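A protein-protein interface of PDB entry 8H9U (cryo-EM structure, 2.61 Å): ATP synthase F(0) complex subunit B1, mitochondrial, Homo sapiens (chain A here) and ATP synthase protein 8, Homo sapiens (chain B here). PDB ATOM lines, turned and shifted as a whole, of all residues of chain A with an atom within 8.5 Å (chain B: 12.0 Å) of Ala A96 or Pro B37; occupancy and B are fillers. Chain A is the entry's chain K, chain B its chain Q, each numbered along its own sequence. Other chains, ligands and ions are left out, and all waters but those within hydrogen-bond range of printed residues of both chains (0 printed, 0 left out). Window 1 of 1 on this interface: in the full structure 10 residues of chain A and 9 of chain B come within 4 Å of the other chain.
Printed residues of chain A that touch a printed residue of chain B: Lys A89, Gln A92, Leu A93 and Ala A96.
Hydrophobic or aromatic side chains of chain A within 4 Å of the printed part of chain B: Leu A93 and Ala A96.
Hydrophobic or aromatic side chains of chain B within 4 Å of the printed part of chain A: His B34, Pro B36 and Pro B37.
Among the printed residues, 4 pairs touch across the chains.
A ring nitrogen (NE2) of His B34 lies close to the side-chain amino group (NZ) of Lys A89.
Among the printed residues, merely in contact across the chains: Gln A92 with Pro B36 (3.3 Å), Leu A93 with Pro B37 (3.4 Å) and Ala A96 with Pro B37 (3.0 Å).
Ala A96 touches just one residue of chain B: Pro B37.
Printed residues of chain A within 4 Å of Pro B37: Leu A93 and Ala A96.
No residue of chain B comes within 4 Å of Glu A94.
No residue of chain B comes within 4 Å of Ala A99.
No residue of chain B comes within 4 Å of Ser A100.
Of the printed residues of chain A, Pro B36 touches Gln A92.
Of the printed residues of chain B, Lys A89 touches His B34.
Of the printed residues of chain A, His B34 touches Lys A89.
Ile A101 touches none of the printed residues of chain B.
Ser B38 touches none of the printed residues of chain A.
The nearest residue of chain B that does not touch Ala A96 is Pro B39 (4.5 Å).
The nearest residue of chain A that does not touch Pro B37 is Gln A92 (4.03 Å).
The nearest printed residue of chain A that does not touch His B34 is Leu A93 (5.0 Å).
O of Ala A96 sits at hydrogen-bond distance from OG of Ser A100, 3.5 Å away.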
ATOM      1  N   LYS A  89     -11.608   0.643  22.456  1.00  0.00           N
ATOM      2  CA  LYS A  89     -11.217  -0.718  22.790  1.00  0.00           C
ATOM      3  C   LYS A  89     -12.296  -1.400  23.616  1.00  0.00           C
ATOM      4  O   LYS A  89     -12.575  -2.589  23.429  1.00  0.00           O
ATOM      5  CB  LYS A  89      -9.890  -0.708  23.539  1.00  0.00           C
ATOM      6  CG  LYS A  89      -9.119  -1.999  23.449  1.00  0.00           C
ATOM      7  CD  LYS A  89      -7.746  -1.830  24.062  1.00  0.00           C
ATOM      8  CE  LYS A  89      -7.005  -3.143  24.096  1.00  0.00           C
ATOM      9  NZ  LYS A  89      -5.709  -3.038  24.816  1.00  0.00           N
ATOM     10  N   LEU A  90     -12.920  -0.660  24.533  1.00  0.00           N
ATOM     11  CA  LEU A  90     -14.021  -1.223  25.302  1.00  0.00           C
ATOM     12  C   LEU A  90     -15.188  -1.587  24.395  1.00  0.00           C
ATOM     13  O   LEU A  90     -15.760  -2.676  24.517  1.00  0.00           O
ATOM     14  CB  LEU A  90     -14.450  -0.236  26.390  1.00  0.00           C
ATOM     15  CG  LEU A  90     -15.708  -0.502  27.216  1.00  0.00           C
ATOM     16  CD1 LEU A  90     -15.523   0.059  28.611  1.00  0.00           C
ATOM     17  CD2 LEU A  90     -16.927   0.130  26.566  1.00  0.00           C
ATOM     18  N   ALA A  91     -15.540  -0.698  23.464  1.00  0.00           N
ATOM     19  CA  ALA A  91     -16.675  -0.959  22.585  1.00  0.00           C
ATOM     20  C   ALA A  91     -16.416  -2.155  21.681  1.00  0.00           C
ATOM     21  O   ALA A  91     -17.279  -3.027  21.534  1.00  0.00           O
ATOM     22  CB  ALA A  91     -16.992   0.280  21.751  1.00  0.00           C
ATOM     23  N   GLN A  92     -15.241  -2.210  21.054  1.00  0.00           N
ATOM     24  CA  GLN A  92     -14.938  -3.326  20.165  1.00  0.00           C
ATOM     25  C   GLN A  92     -14.942  -4.644  20.924  1.00  0.00           C
ATOM     26  O   GLN A  92     -15.364  -5.679  20.396  1.00  0.00           O
ATOM     27  CB  GLN A  92     -13.591  -3.107  19.481  1.00  0.00           C
ATOM     28  CG  GLN A  92     -13.130  -4.299  18.661  1.00  0.00           C
ATOM     29  CD  GLN A  92     -11.674  -4.205  18.253  1.00  0.00           C
ATOM     30  OE1 GLN A  92     -11.015  -3.194  18.486  1.00  0.00           O
ATOM     31  NE2 GLN A  92     -11.164  -5.267  17.644  1.00  0.00           N
ATOM     32  N   LEU A  93     -14.481  -4.628  22.174  1.00  0.00           N
ATOM     33  CA  LEU A  93     -14.417  -5.863  22.945  1.00  0.00           C
ATOM     34  C   LEU A  93     -15.807  -6.360  23.313  1.00  0.00           C
ATOM     35  O   LEU A  93     -16.169  -7.502  23.009  1.00  0.00           O
ATOM     36  CB  LEU A  93     -13.570  -5.654  24.195  1.00  0.00           C
ATOM     37  CG  LEU A  93     -12.071  -5.607  23.932  1.00  0.00           C
ATOM     38  CD1 LEU A  93     -11.355  -5.437  25.234  1.00  0.00           C
ATOM     39  CD2 LEU A  93     -11.610  -6.866  23.238  1.00  0.00           C
ATOM     40  N   GLU A  94     -16.600  -5.517  23.982  1.00  0.00           N
ATOM     41  CA  GLU A  94     -17.950  -5.923  24.361  1.00  0.00           C
ATOM     42  C   GLU A  94     -18.760  -6.359  23.149  1.00  0.00           C
ATOM     43  O   GLU A  94     -19.643  -7.215  23.266  1.00  0.00           O
ATOM     44  CB  GLU A  94     -18.655  -4.787  25.102  1.00  0.00           C
ATOM     45  CG  GLU A  94     -18.852  -3.525  24.281  1.00  0.00           C
ATOM     46  CD  GLU A  94     -20.095  -3.579  23.414  1.00  0.00           C
ATOM     47  OE1 GLU A  94     -21.103  -4.171  23.853  1.00  0.00           O
ATOM     48  OE2 GLU A  94     -20.059  -3.045  22.287  1.00  0.00           O
ATOM     49  N   GLU A  95     -18.475  -5.785  21.980  1.00  0.00           N
ATOM     50  CA  GLU A  95     -19.116  -6.252  20.760  1.00  0.00           C
ATOM     51  C   GLU A  95     -18.754  -7.699  20.466  1.00  0.00           C
ATOM     52  O   GLU A  95     -19.644  -8.516  20.206  1.00  0.00           O
ATOM     53  CB  GLU A  95     -18.723  -5.361  19.589  1.00  0.00           C
ATOM     54  CG  GLU A  95     -18.800  -6.048  18.247  1.00  0.00           C
ATOM     55  CD  GLU A  95     -18.692  -5.071  17.102  1.00  0.00           C
ATOM     56  OE1 GLU A  95     -19.686  -4.368  16.827  1.00  0.00           O
ATOM     57  OE2 GLU A  95     -17.613  -5.002  16.479  1.00  0.00           O
ATOM     58  N   ALA A  96     -17.471  -8.039  20.518  1.00  0.00           N
ATOM     59  CA  ALA A  96     -17.049  -9.420  20.349  1.00  0.00           C
ATOM     60  C   ALA A  96     -17.446 -10.299  21.523  1.00  0.00           C
ATOM     61  O   ALA A  96     -17.206 -11.509  21.481  1.00  0.00           O
ATOM     62  CB  ALA A  96     -15.539  -9.488  20.133  1.00  0.00           C
ATOM     63  N   LYS A  97     -18.033  -9.724  22.570  1.00  0.00           N
ATOM     64  CA  LYS A  97     -18.735 -10.514  23.568  1.00  0.00           C
ATOM     65  C   LYS A  97     -20.140 -10.878  23.123  1.00  0.00           C
ATOM     66  O   LYS A  97     -20.585 -12.002  23.373  1.00  0.00           O
ATOM     67  CB  LYS A  97     -18.803  -9.764  24.903  1.00  0.00           C
ATOM     68  CG  LYS A  97     -19.496 -10.538  26.010  1.00  0.00           C
ATOM     69  CD  LYS A  97     -19.450  -9.797  27.333  1.00  0.00           C
ATOM     70  CE  LYS A  97     -18.117 -10.005  28.030  1.00  0.00           C
ATOM     71  NZ  LYS A  97     -18.129  -9.533  29.442  1.00  0.00           N
ATOM     72  N   GLN A  98     -20.836  -9.964  22.448  1.00  0.00           N
ATOM     73  CA  GLN A  98     -22.146 -10.289  21.898  1.00  0.00           C
ATOM     74  C   GLN A  98     -22.036 -11.296  20.763  1.00  0.00           C
ATOM     75  O   GLN A  98     -22.828 -12.240  20.691  1.00  0.00           O
ATOM     76  CB  GLN A  98     -22.843  -9.022  21.408  1.00  0.00           C
ATOM     77  CG  GLN A  98     -22.832  -7.887  22.406  1.00  0.00           C
ATOM     78  CD  GLN A  98     -23.092  -8.356  23.820  1.00  0.00           C
ATOM     79  OE1 GLN A  98     -22.194  -8.350  24.662  1.00  0.00           O
ATOM     80  NE2 GLN A  98     -24.324  -8.769  24.091  1.00  0.00           N
ATOM     81  N   ALA A  99     -21.055 -11.114  19.876  1.00  0.00           N
ATOM     82  CA  ALA A  99     -20.944 -11.978  18.707  1.00  0.00           C
ATOM     83  C   ALA A  99     -20.737 -13.432  19.105  1.00  0.00           C
ATOM     84  O   ALA A  99     -21.130 -14.344  18.368  1.00  0.00           O
ATOM     85  CB  ALA A  99     -19.811 -11.500  17.805  1.00  0.00           C
ATOM     86  N   SER A 100     -20.121 -13.674  20.262  1.00  0.00           N
ATOM     87  CA  SER A 100     -20.085 -15.036  20.782  1.00  0.00           C
ATOM     88  C   SER A 100     -21.477 -15.500  21.176  1.00  0.00           C
ATOM     89  O   SER A 100     -21.938 -16.553  20.721  1.00  0.00           O
ATOM     90  CB  SER A 100     -19.143 -15.132  21.980  1.00  0.00           C
ATOM     91  OG  SER A 100     -17.798 -14.918  21.604  1.00  0.00           O
ATOM     92  N   ILE A 101     -22.161 -14.715  22.013  1.00  0.00           N
ATOM     93  CA  ILE A 101     -23.492 -15.078  22.487  1.00  0.00           C
ATOM     94  C   ILE A 101     -24.399 -15.433  21.318  1.00  0.00           C
ATOM     95  O   ILE A 101     -25.029 -16.496  21.295  1.00  0.00           O
ATOM     96  CB  ILE A 101     -24.085 -13.935  23.327  1.00  0.00           C
ATOM     97  CG1 ILE A 101     -23.103 -13.528  24.423  1.00  0.00           C
ATOM     98  CG2 ILE A 101     -25.424 -14.344  23.917  1.00  0.00           C
ATOM     99  CD1 ILE A 101     -23.689 -12.605  25.462  1.00  0.00           C
ATOM    100  N   GLN A 102     -24.461 -14.555  20.317  1.00  0.00           N
ATOM    101  CA  GLN A 102     -25.373 -14.781  19.202  1.00  0.00           C
ATOM    102  C   GLN A 102     -24.987 -16.018  18.403  1.00  0.00           C
ATOM    103  O   GLN A 102     -25.865 -16.753  17.939  1.00  0.00           O
ATOM    104  CB  GLN A 102     -25.414 -13.550  18.304  1.00  0.00           C
ATOM    105  CG  GLN A 102     -25.695 -12.273  19.055  1.00  0.00           C
ATOM    106  CD  GLN A 102     -26.189 -11.176  18.146  1.00  0.00           C
ATOM    107  OE1 GLN A 102     -26.585 -10.107  18.606  1.00  0.00           O
ATOM    108  NE2 GLN A 102     -26.176 -11.434  16.845  1.00  0.00           N
ATOM    109  N   TYR B  33       0.761  -6.453  22.480  1.00  0.00           N
ATOM    110  CA  TYR B  33      -0.420  -6.081  21.661  1.00  0.00           C
ATOM    111  C   TYR B  33      -1.153  -7.366  21.267  1.00  0.00           C
ATOM    112  O   TYR B  33      -0.597  -8.150  20.478  1.00  0.00           O
ATOM    113  CB  TYR B  33       0.022  -5.257  20.450  1.00  0.00           C
ATOM    114  CG  TYR B  33       0.741  -3.979  20.797  1.00  0.00           C
ATOM    115  CD1 TYR B  33       0.097  -2.955  21.472  1.00  0.00           C
ATOM    116  CD2 TYR B  33       2.075  -3.796  20.471  1.00  0.00           C
ATOM    117  CE1 TYR B  33       0.751  -1.778  21.797  1.00  0.00           C
ATOM    118  CE2 TYR B  33       2.745  -2.625  20.789  1.00  0.00           C
ATOM    119  CZ  TYR B  33       2.081  -1.611  21.455  1.00  0.00           C
ATOM    120  OH  TYR B  33       2.738  -0.449  21.776  1.00  0.00           O
ATOM    121  N   HIS B  34      -2.352  -7.581  21.807  1.00  0.00           N
ATOM    122  CA  HIS B  34      -3.117  -8.785  21.551  1.00  0.00           C
ATOM    123  C   HIS B  34      -3.842  -8.687  20.214  1.00  0.00           C
ATOM    124  O   HIS B  34      -4.271  -7.613  19.783  1.00  0.00           O
ATOM    125  CB  HIS B  34      -4.125  -9.007  22.665  1.00  0.00           C
ATOM    126  CG  HIS B  34      -5.062  -7.861  22.840  1.00  0.00           C
ATOM    127  ND1 HIS B  34      -6.062  -7.575  21.936  1.00  0.00           N
ATOM    128  CD2 HIS B  34      -5.138  -6.909  23.797  1.00  0.00           C
ATOM    129  CE1 HIS B  34      -6.723  -6.505  22.338  1.00  0.00           C
ATOM    130  NE2 HIS B  34      -6.183  -6.084  23.466  1.00  0.00           N
ATOM    131  N   LEU B  35      -3.990  -9.827  19.566  1.00  0.00           N
ATOM    132  CA  LEU B  35      -4.767  -9.884  18.339  1.00  0.00           C
ATOM    133  C   LEU B  35      -6.226  -9.579  18.657  1.00  0.00           C
ATOM    134  O   LEU B  35      -6.770 -10.130  19.617  1.00  0.00           O
ATOM    135  CB  LEU B  35      -4.646 -11.256  17.688  1.00  0.00           C
ATOM    136  CG  LEU B  35      -3.265 -11.686  17.188  1.00  0.00           C
ATOM    137  CD1 LEU B  35      -2.391 -12.203  18.316  1.00  0.00           C
ATOM    138  CD2 LEU B  35      -3.400 -12.744  16.112  1.00  0.00           C
ATOM    139  N   PRO B  36      -6.880  -8.710  17.898  1.00  0.00           N
ATOM    140  CA  PRO B  36      -8.237  -8.285  18.254  1.00  0.00           C
ATOM    141  C   PRO B  36      -9.223  -9.428  18.101  1.00  0.00           C
ATOM    142  O   PRO B  36      -9.048 -10.300  17.237  1.00  0.00           O
ATOM    143  CB  PRO B  36      -8.532  -7.158  17.253  1.00  0.00           C
ATOM    144  CG  PRO B  36      -7.210  -6.804  16.646  1.00  0.00           C
ATOM    145  CD  PRO B  36      -6.407  -8.057  16.671  1.00  0.00           C
ATOM    146  N   PRO B  37     -10.273  -9.498  18.954  1.00  0.00           N
ATOM    147  CA  PRO B  37     -11.188 -10.644  18.942  1.00  0.00           C
ATOM    148  C   PRO B  37     -12.347 -10.574  17.940  1.00  0.00           C
ATOM    149  O   PRO B  37     -13.298  -9.861  18.196  1.00  0.00           O
ATOM    150  CB  PRO B  37     -11.762 -10.606  20.366  1.00  0.00           C
ATOM    151  CG  PRO B  37     -11.828  -9.132  20.695  1.00  0.00           C
ATOM    152  CD  PRO B  37     -10.649  -8.510  19.975  1.00  0.00           C
ATOM    153  N   SER B  38     -12.237 -11.302  16.828  1.00  0.00           N
ATOM    154  CA  SER B  38     -13.371 -11.403  15.875  1.00  0.00           C
ATOM    155  C   SER B  38     -13.671 -12.893  15.729  1.00  0.00           C
ATOM    156  O   SER B  38     -13.768 -13.342  14.574  1.00  0.00           O
ATOM    157  CB  SER B  38     -13.036 -10.765  14.556  1.00  0.00           C
ATOM    158  OG  SER B  38     -11.898 -11.384  13.973  1.00  0.00           O
ATOM    159  N   PRO B  39     -13.942 -13.672  16.803  1.00  0.00           N
ATOM    160  CA  PRO B  39     -14.341 -15.075  16.640  1.00  0.00           C
ATOM    161  C   PRO B  39     -15.530 -15.144  15.670  1.00  0.00           C
ATOM    162  O   PRO B  39     -16.551 -14.551  15.971  1.00  0.00           O
ATOM    163  CB  PRO B  39     -14.769 -15.505  18.048  1.00  0.00           C
ATOM    164  CG  PRO B  39     -13.982 -14.596  18.962  1.00  0.00           C
ATOM    165  CD  PRO B  39     -13.911 -13.278  18.219  1.00  0.00           C
ATOM    166  N   LYS B  40     -15.378 -15.852  14.548  1.00  0.00           N
ATOM    167  CA  LYS B  40     -16.453 -15.904  13.515  1.00  0.00           C
ATOM    168  C   LYS B  40     -17.707 -16.583  14.077  1.00  0.00           C
ATOM    169  O   LYS B  40     -17.563 -17.606  14.774  1.00  0.00           O
ATOM    170  CB  LYS B  40     -15.950 -16.639  12.270  1.00  0.00           C
ATOM    171  CG  LYS B  40     -16.993 -16.868  11.183  1.00  0.00           C
ATOM    172  CD  LYS B  40     -16.419 -17.490   9.930  1.00  0.00           C
ATOM    173  CE  LYS B  40     -15.631 -18.752  10.205  1.00  0.00           C
ATOM    174  NZ  LYS B  40     -15.116 -19.360   8.956  1.00  0.00           N
ATOM    175  N   PRO B  41     -18.925 -16.067  13.798  1.00  0.00           N
ATOM    176  CA  PRO B  41     -20.167 -16.711  14.242  1.00  0.00           C
ATOM    177  C   PRO B  41     -20.537 -17.878  13.317  1.00  0.00           C
ATOM    178  O   PRO B  41     -21.684 -18.284  13.328  1.00  0.00           O
ATOM    179  CB  PRO B  41     -21.197 -15.583  14.108  1.00  0.00           C
ATOM    180  CG  PRO B  41     -20.689 -14.774  12.937  1.00  0.00           C
ATOM    181  CD  PRO B  41     -19.178 -14.831  13.051  1.00  0.00           C
ATOM    182  N   MET B  42     -19.573 -18.371  12.536  1.00  0.00           N
ATOM    183  CA  MET B  42     -19.810 -19.508  11.648  1.00  0.00           C
ATOM    184  C   MET B  42     -18.773 -20.583  11.958  1.00  0.00           C
ATOM    185  O   MET B  42     -17.732 -20.661  11.300  1.00  0.00           O
ATOM    186  CB  MET B  42     -19.751 -19.075  10.186  1.00  0.00           C
ATOM    187  CG  MET B  42     -20.465 -20.007   9.216  1.00  0.00           C
ATOM    188  SD  MET B  42     -22.200 -20.289   9.622  1.00  0.00           S
ATOM    189  CE  MET B  42     -22.130 -21.945  10.296  1.00  0.00           C
